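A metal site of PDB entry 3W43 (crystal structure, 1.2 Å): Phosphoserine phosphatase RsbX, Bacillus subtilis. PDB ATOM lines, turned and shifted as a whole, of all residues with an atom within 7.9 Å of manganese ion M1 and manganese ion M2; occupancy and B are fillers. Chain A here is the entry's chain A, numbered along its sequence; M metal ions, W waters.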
ATOM      1  N   LYS A  19     -20.538 -23.725  -7.174  1.00  0.00           N
ATOM      2  CA  LYS A  19     -19.502 -23.538  -8.154  1.00  0.00           C
ATOM      3  C   LYS A  19     -19.504 -24.713  -9.141  1.00  0.00           C
ATOM      4  O   LYS A  19     -19.814 -25.854  -8.784  1.00  0.00           O
ATOM      5  CB  LYS A  19     -18.157 -23.480  -7.454  1.00  0.00           C
ATOM      6  CG  LYS A  19     -17.023 -23.173  -8.382  1.00  0.00           C
ATOM      7  CD  LYS A  19     -15.730 -23.035  -7.651  1.00  0.00           C
ATOM      8  CE  LYS A  19     -14.648 -22.628  -8.625  1.00  0.00           C
ATOM      9  NZ  LYS A  19     -13.426 -22.246  -7.892  1.00  0.00           N
ATOM     10  N   CYS A  25     -21.786 -27.353  -1.579  1.00  0.00           N
ATOM     11  CA  CYS A  25     -21.565 -25.924  -1.592  1.00  0.00           C
ATOM     12  C   CYS A  25     -20.645 -25.478  -0.479  1.00  0.00           C
ATOM     13  O   CYS A  25     -20.788 -25.883   0.677  1.00  0.00           O
ATOM     14  CB  CYS A  25     -22.907 -25.207  -1.471  1.00  0.00           C
ATOM     15  SG  CYS A  25     -22.846 -23.466  -1.949  1.00  0.00           S
ATOM     16  N   GLY A  26     -19.671 -24.640  -0.825  1.00  0.00           N
ATOM     17  CA  GLY A  26     -18.820 -24.030   0.187  1.00  0.00           C
ATOM     18  C   GLY A  26     -19.509 -22.944   0.989  1.00  0.00           C
ATOM     19  O   GLY A  26     -19.039 -22.599   2.068  1.00  0.00           O
ATOM     20  N   ASP A  27     -20.618 -22.410   0.472  1.00  0.00           N
ATOM     21  CA  ASP A  27     -21.436 -21.448   1.212  1.00  0.00           C
ATOM     22  C   ASP A  27     -22.453 -22.213   2.051  1.00  0.00           C
ATOM     23  O   ASP A  27     -22.924 -23.280   1.612  1.00  0.00           O
ATOM     24  CB  ASP A  27     -22.281 -20.577   0.264  1.00  0.00           C
ATOM     25  CG  ASP A  27     -21.478 -19.628  -0.630  1.00  0.00           C
ATOM     26  OD1 ASP A  27     -20.237 -19.452  -0.488  1.00  0.00           O
ATOM     27  OD2 ASP A  27     -22.164 -19.050  -1.510  1.00  0.00           O
ATOM     28  N   ALA A  43     -22.835 -17.689   5.211  1.00  0.00           N
ATOM     29  CA  ALA A  43     -21.394 -17.865   5.375  1.00  0.00           C
ATOM     30  C   ALA A  43     -20.767 -18.450   4.125  1.00  0.00           C
ATOM     31  O   ALA A  43     -21.340 -19.305   3.462  1.00  0.00           O
ATOM     32  CB  ALA A  43     -21.115 -18.764   6.566  1.00  0.00           C
ATOM     33  N   ASP A  44     -19.565 -17.973   3.808  1.00  0.00           N
ATOM     34  CA  ASP A  44     -18.815 -18.433   2.652  1.00  0.00           C
ATOM     35  C   ASP A  44     -17.491 -19.015   3.165  1.00  0.00           C
ATOM     36  O   ASP A  44     -16.623 -18.292   3.606  1.00  0.00           O
ATOM     37  CB  ASP A  44     -18.578 -17.226   1.734  1.00  0.00           C
ATOM     38  CG  ASP A  44     -17.771 -17.582   0.491  1.00  0.00           C
ATOM     39  OD1 ASP A  44     -17.307 -18.742   0.404  1.00  0.00           O
ATOM     40  OD2 ASP A  44     -17.617 -16.721  -0.402  1.00  0.00           O
ATOM     41  N   GLY A  45     -17.392 -20.349   3.159  1.00  0.00           N
ATOM     42  CA  GLY A  45     -16.170 -21.005   3.623  1.00  0.00           C
ATOM     43  C   GLY A  45     -15.055 -20.730   2.635  1.00  0.00           C
ATOM     44  O   GLY A  45     -15.290 -20.670   1.443  1.00  0.00           O
ATOM     45  N   LEU A  46     -13.852 -20.541   3.143  1.00  0.00           N
ATOM     46  CA  LEU A  46     -12.720 -20.279   2.244  1.00  0.00           C
ATOM     47  C   LEU A  46     -12.555 -21.391   1.221  1.00  0.00           C
ATOM     48  O   LEU A  46     -12.651 -22.571   1.545  1.00  0.00           O
ATOM     49  CB  LEU A  46     -11.447 -20.061   3.038  1.00  0.00           C
ATOM     50  CG  LEU A  46     -11.143 -18.603   3.383  1.00  0.00           C
ATOM     51  CD1 LEU A  46     -12.230 -17.892   4.173  1.00  0.00           C
ATOM     52  CD2 LEU A  46      -9.808 -18.531   4.098  1.00  0.00           C
ATOM     53  N   GLY A  47     -12.325 -20.992  -0.030  1.00  0.00           N
ATOM     54  CA  GLY A  47     -12.271 -21.934  -1.132  1.00  0.00           C
ATOM     55  C   GLY A  47     -13.659 -22.375  -1.529  1.00  0.00           C
ATOM     56  O   GLY A  47     -14.633 -21.596  -1.466  1.00  0.00           O
ATOM     57  N   SER A  48     -13.779 -23.636  -1.917  1.00  0.00           N
ATOM     58  CA  SER A  48     -15.064 -24.184  -2.353  1.00  0.00           C
ATOM     59  C   SER A  48     -15.141 -25.643  -1.935  1.00  0.00           C
ATOM     60  O   SER A  48     -14.222 -26.172  -1.333  1.00  0.00           O
ATOM     61  CB  SER A  48     -15.261 -24.030  -3.861  1.00  0.00           C
ATOM     62  OG  SER A  48     -14.294 -24.769  -4.595  1.00  0.00           O
ATOM     63  N   GLY A  49     -16.259 -26.290  -2.242  1.00  0.00           N
ATOM     64  CA  GLY A  49     -16.374 -27.731  -2.026  1.00  0.00           C
ATOM     65  C   GLY A  49     -16.373 -28.137  -0.572  1.00  0.00           C
ATOM     66  O   GLY A  49     -16.753 -27.363   0.313  1.00  0.00           O
ATOM     67  N   ALA A  52     -14.448 -26.028   2.218  1.00  0.00           N
ATOM     68  CA  ALA A  52     -15.152 -24.763   2.488  1.00  0.00           C
ATOM     69  C   ALA A  52     -16.399 -25.029   3.314  1.00  0.00           C
ATOM     70  O   ALA A  52     -16.691 -24.309   4.287  1.00  0.00           O
ATOM     71  CB  ALA A  52     -15.514 -24.114   1.181  1.00  0.00           C
ATOM     72  N   ASN A  53     -17.132 -26.083   2.941  1.00  0.00           N
ATOM     73  CA  ASN A  53     -18.351 -26.463   3.624  1.00  0.00           C
ATOM     74  C   ASN A  53     -18.090 -26.819   5.090  1.00  0.00           C
ATOM     75  O   ASN A  53     -18.893 -26.494   5.953  1.00  0.00           O
ATOM     76  CB  ASN A  53     -19.050 -27.605   2.887  1.00  0.00           C
ATOM     77  CG  ASN A  53     -20.358 -27.981   3.529  1.00  0.00           C
ATOM     78  OD1 ASN A  53     -20.400 -28.847   4.390  1.00  0.00           O
ATOM     79  ND2 ASN A  53     -21.430 -27.301   3.143  1.00  0.00           N
ATOM     80  N   SER A  56     -18.219 -23.349   6.714  1.00  0.00           N
ATOM     81  CA  SER A  56     -19.500 -22.641   6.688  1.00  0.00           C
ATOM     82  C   SER A  56     -20.626 -23.418   7.360  1.00  0.00           C
ATOM     83  O   SER A  56     -21.505 -22.821   7.974  1.00  0.00           O
ATOM     84  CB  SER A  56     -19.869 -22.231   5.267  1.00  0.00           C
ATOM     85  OG  SER A  56     -20.091 -23.372   4.455  1.00  0.00           O
ATOM     86  N   ARG A  86     -10.534 -24.163   7.682  1.00  0.00           N
ATOM     87  CA  ARG A  86     -10.101 -23.159   6.711  1.00  0.00           C
ATOM     88  C   ARG A  86     -10.513 -21.759   7.158  1.00  0.00           C
ATOM     89  O   ARG A  86      -9.766 -20.796   6.991  1.00  0.00           O
ATOM     90  CB  ARG A  86     -10.676 -23.426   5.322  1.00  0.00           C
ATOM     91  CG  ARG A  86      -9.950 -24.472   4.499  1.00  0.00           C
ATOM     92  CD  ARG A  86     -10.540 -24.530   3.102  1.00  0.00           C
ATOM     93  NE  ARG A  86      -9.777 -25.328   2.158  1.00  0.00           N
ATOM     94  CZ  ARG A  86     -10.144 -25.523   0.890  1.00  0.00           C
ATOM     95  NH1 ARG A  86     -11.271 -24.995   0.444  1.00  0.00           N
ATOM     96  NH2 ARG A  86      -9.409 -26.266   0.084  1.00  0.00           N
ATOM     97  N   GLY A  87     -11.726 -21.654   7.709  1.00  0.00           N
ATOM     98  CA  GLY A  87     -12.285 -20.350   8.030  1.00  0.00           C
ATOM     99  C   GLY A  87     -13.352 -19.932   7.048  1.00  0.00           C
ATOM    100  O   GLY A  87     -13.595 -20.629   6.053  1.00  0.00           O
ATOM    101  N   ALA A  88     -14.000 -18.801   7.314  1.00  0.00           N
ATOM    102  CA  ALA A  88     -15.128 -18.381   6.499  1.00  0.00           C
ATOM    103  C   ALA A  88     -15.357 -16.899   6.648  1.00  0.00           C
ATOM    104  O   ALA A  88     -14.971 -16.310   7.656  1.00  0.00           O
ATOM    105  CB  ALA A  88     -16.396 -19.132   6.921  1.00  0.00           C
ATOM    106  N   THR A  89     -16.024 -16.305   5.659  1.00  0.00           N
ATOM    107  CA  THR A  89     -16.613 -14.985   5.808  1.00  0.00           C
ATOM    108  C   THR A  89     -18.102 -15.176   6.148  1.00  0.00           C
ATOM    109  O   THR A  89     -18.689 -16.209   5.811  1.00  0.00           O
ATOM    110  CB  THR A  89     -16.411 -14.152   4.535  1.00  0.00           C
ATOM    111  OG1 THR A  89     -16.993 -14.859   3.425  1.00  0.00           O
ATOM    112  CG2 THR A  89     -14.915 -13.952   4.269  1.00  0.00           C
ATOM    113  N   ASN A 109     -16.354 -10.606   2.728  1.00  0.00           N
ATOM    114  CA  ASN A 109     -17.157 -10.144   1.602  1.00  0.00           C
ATOM    115  C   ASN A 109     -18.485 -10.886   1.437  1.00  0.00           C
ATOM    116  O   ASN A 109     -18.770 -11.501   0.401  1.00  0.00           O
ATOM    117  CB  ASN A 109     -16.344 -10.212   0.288  1.00  0.00           C
ATOM    118  CG  ASN A 109     -16.976  -9.402  -0.841  1.00  0.00           C
ATOM    119  OD1 ASN A 109     -17.867  -8.566  -0.619  1.00  0.00           O
ATOM    120  ND2 ASN A 109     -16.511  -9.635  -2.071  1.00  0.00           N
ATOM    121  N   VAL A 110     -19.307 -10.839   2.487  1.00  0.00           N
ATOM    122  CA  VAL A 110     -20.705 -11.201   2.410  1.00  0.00           C
ATOM    123  C   VAL A 110     -21.426  -9.870   2.615  1.00  0.00           C
ATOM    124  O   VAL A 110     -21.143  -9.154   3.584  1.00  0.00           O
ATOM    125  CB  VAL A 110     -21.087 -12.241   3.496  1.00  0.00           C
ATOM    126  CG1 VAL A 110     -22.554 -12.634   3.371  1.00  0.00           C
ATOM    127  CG2 VAL A 110     -20.211 -13.505   3.401  1.00  0.00           C
ATOM    128  N   THR A 155     -23.500 -13.880  -0.853  1.00  0.00           N
ATOM    129  CA  THR A 155     -22.079 -14.151  -0.972  1.00  0.00           C
ATOM    130  C   THR A 155     -21.492 -13.541  -2.232  1.00  0.00           C
ATOM    131  O   THR A 155     -22.202 -13.058  -3.126  1.00  0.00           O
ATOM    132  CB  THR A 155     -21.761 -15.660  -0.901  1.00  0.00           C
ATOM    133  OG1 THR A 155     -22.386 -16.333  -2.012  1.00  0.00           O
ATOM    134  CG2 THR A 155     -22.238 -16.252   0.415  1.00  0.00           C
ATOM    135  N   ASP A 156     -20.163 -13.549  -2.283  1.00  0.00           N
ATOM    136  CA  ASP A 156     -19.419 -12.914  -3.362  1.00  0.00           C
ATOM    137  C   ASP A 156     -19.526 -13.639  -4.706  1.00  0.00           C
ATOM    138  O   ASP A 156     -19.051 -13.142  -5.706  1.00  0.00           O
ATOM    139  CB  ASP A 156     -17.963 -12.681  -2.927  1.00  0.00           C
ATOM    140  CG  ASP A 156     -17.230 -13.969  -2.583  1.00  0.00           C
ATOM    141  OD1 ASP A 156     -17.709 -15.061  -2.947  1.00  0.00           O
ATOM    142  OD2 ASP A 156     -16.143 -13.874  -1.944  1.00  0.00           O
ATOM    143  N   GLY A 157     -20.161 -14.806  -4.737  1.00  0.00           N
ATOM    144  CA  GLY A 157     -20.495 -15.441  -5.996  1.00  0.00           C
ATOM    145  C   GLY A 157     -21.504 -14.630  -6.782  1.00  0.00           C
ATOM    146  O   GLY A 157     -21.618 -14.795  -7.981  1.00  0.00           O
ATOM    147  N   LEU A 158     -22.264 -13.773  -6.101  1.00  0.00           N
ATOM    148  CA  LEU A 158     -23.210 -12.865  -6.739  1.00  0.00           C
ATOM    149  C   LEU A 158     -22.557 -11.495  -6.841  1.00  0.00           C
ATOM    150  O   LEU A 158     -22.247 -10.860  -5.820  1.00  0.00           O
ATOM    151  CB  LEU A 158     -24.523 -12.787  -5.957  1.00  0.00           C
ATOM    152  CG  LEU A 158     -25.593 -11.859  -6.548  1.00  0.00           C
ATOM    153  CD1 LEU A 158     -26.154 -12.463  -7.817  1.00  0.00           C
ATOM    154  CD2 LEU A 158     -26.711 -11.604  -5.566  1.00  0.00           C
ATOM    155  N   LYS A 188     -19.118 -19.499 -11.612  1.00  0.00           N
ATOM    156  CA  LYS A 188     -17.705 -19.244 -11.367  1.00  0.00           C
ATOM    157  C   LYS A 188     -17.342 -19.452  -9.905  1.00  0.00           C
ATOM    158  O   LYS A 188     -16.200 -19.793  -9.586  1.00  0.00           O
ATOM    159  CB  LYS A 188     -17.277 -17.854 -11.846  1.00  0.00           C
ATOM    160  CG  LYS A 188     -17.237 -17.683 -13.362  1.00  0.00           C
ATOM    161  CD  LYS A 188     -16.706 -16.310 -13.762  1.00  0.00           C
ATOM    162  CE  LYS A 188     -15.191 -16.200 -13.638  1.00  0.00           C
ATOM    163  NZ  LYS A 188     -14.458 -17.054 -14.628  1.00  0.00           N
ATOM    164  N   ASP A 189     -18.312 -19.246  -9.030  1.00  0.00           N
ATOM    165  CA  ASP A 189     -18.126 -19.481  -7.604  1.00  0.00           C
ATOM    166  C   ASP A 189     -19.443 -19.962  -7.040  1.00  0.00           C
ATOM    167  O   ASP A 189     -20.483 -19.800  -7.674  1.00  0.00           O
ATOM    168  CB  ASP A 189     -17.709 -18.161  -6.923  1.00  0.00           C
ATOM    169  CG  ASP A 189     -17.290 -18.343  -5.474  1.00  0.00           C
ATOM    170  OD1 ASP A 189     -17.017 -19.502  -5.053  1.00  0.00           O
ATOM    171  OD2 ASP A 189     -17.219 -17.320  -4.754  1.00  0.00           O
ATOM    172  N   ASP A 190     -19.408 -20.543  -5.848  1.00  0.00           N
ATOM    173  CA  ASP A 190     -20.615 -20.750  -5.058  1.00  0.00           C
ATOM    174  C   ASP A 190     -21.352 -19.422  -4.968  1.00  0.00           C
ATOM    175  O   ASP A 190     -20.747 -18.368  -4.760  1.00  0.00           O
ATOM    176  CB  ASP A 190     -20.268 -21.220  -3.643  1.00  0.00           C
ATOM    177  CG  ASP A 190     -19.622 -22.601  -3.612  1.00  0.00           C
ATOM    178  OD1 ASP A 190     -20.038 -23.499  -4.380  1.00  0.00           O
ATOM    179  OD2 ASP A 190     -18.709 -22.794  -2.789  1.00  0.00           O
ATOM    180  N   LEU A 191     -22.673 -19.487  -5.081  1.00  0.00           N
ATOM    181  CA  LEU A 191     -23.498 -18.288  -5.076  1.00  0.00           C
ATOM    182  C   LEU A 191     -24.718 -18.516  -4.189  1.00  0.00           C
ATOM    183  O   LEU A 191     -25.492 -19.449  -4.437  1.00  0.00           O
ATOM    184  CB  LEU A 191     -23.910 -17.959  -6.517  1.00  0.00           C
ATOM    185  CG  LEU A 191     -24.579 -16.631  -6.820  1.00  0.00           C
ATOM    186  CD1 LEU A 191     -24.532 -16.380  -8.305  1.00  0.00           C
ATOM    187  CD2 LEU A 191     -26.005 -16.610  -6.311  1.00  0.00           C
ATOM    188  N   THR A 192     -24.870 -17.689  -3.157  1.00  0.00           N
ATOM    189  CA  THR A 192     -25.975 -17.791  -2.206  1.00  0.00           C
ATOM    190  C   THR A 192     -26.543 -16.409  -1.969  1.00  0.00           C
ATOM    191  O   THR A 192     -25.787 -15.463  -1.727  1.00  0.00           O
ATOM    192  CB  THR A 192     -25.486 -18.349  -0.856  1.00  0.00           C
ATOM    193  OG1 THR A 192     -24.816 -19.590  -1.068  1.00  0.00           O
ATOM    194  CG2 THR A 192     -26.647 -18.595   0.099  1.00  0.00           C
HETATM  195 MN    MN M   1     -15.942 -20.015  -0.615  1.00  0.00          MN
HETATM  196 MN    MN M   2     -17.223 -17.094  -2.505  1.00  0.00          MN
HETATM  197  O   HOH W   1     -19.274 -17.849  -2.536  1.00  0.00           O
HETATM  198  O   HOH W   2     -17.887 -21.063  -0.929  1.00  0.00           O
HETATM  199  O   HOH W   3     -16.268 -19.075  -2.529  1.00  0.00           O
HETATM  200  O   HOH W   4     -15.140 -16.318  -2.294  1.00  0.00           O
HETATM  201  O   HOH W   5     -14.456 -18.268  -0.417  1.00  0.00           O
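Water W2 lies within hydrogen-bond range of the side-chain carboxylate of Asp 190 (2.7 Å) and the side-chain carboxylate of Asp 27 (2.9 Å). Water W1 lies within hydrogen-bond range of the backbone carbonyl oxygen of Asp 190 (2.7 Å) and the side-chain carboxylate of Asp 27 (2.8 Å).
Manganese ion M2 is bound by the side-chain carboxylate of Asp 156 (2.1 Å), the side-chain carboxylate of Asp 44 (2.2 Å), water W1 (2.2 Å), water W3 (2.2 Å), water W4 (2.2 Å) and the side-chain carboxylate of Asp 189 (2.3 Å).
OD1 of Asp 44 binds manganese ion M1 (2.1 Å). Manganese ion M1 is bound by water W3 (2.2 Å). The backbone carbonyl oxygen (O) of Gly 47 binds manganese ion M1. Water W2 is bound to manganese ion M1 (2.2 Å). O of Gly 45 binds manganese ion M1 (2.3 Å). Water W5 is bound to manganese ion M1, 2.3 Å away. Manganese ion M1 has six donor atoms within binding distance.
The backbone NH of Gly 45 lies within hydrogen-bond range of the backbone carbonyl oxygen of Gly 26, at 3.0 Å. N of Asp 44 is in hydrogen-bond range of O of Thr 89 (2.8 Å).
Within 4 Å of manganese ion M2: Asp 44, Asp 156 and Asp 189.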
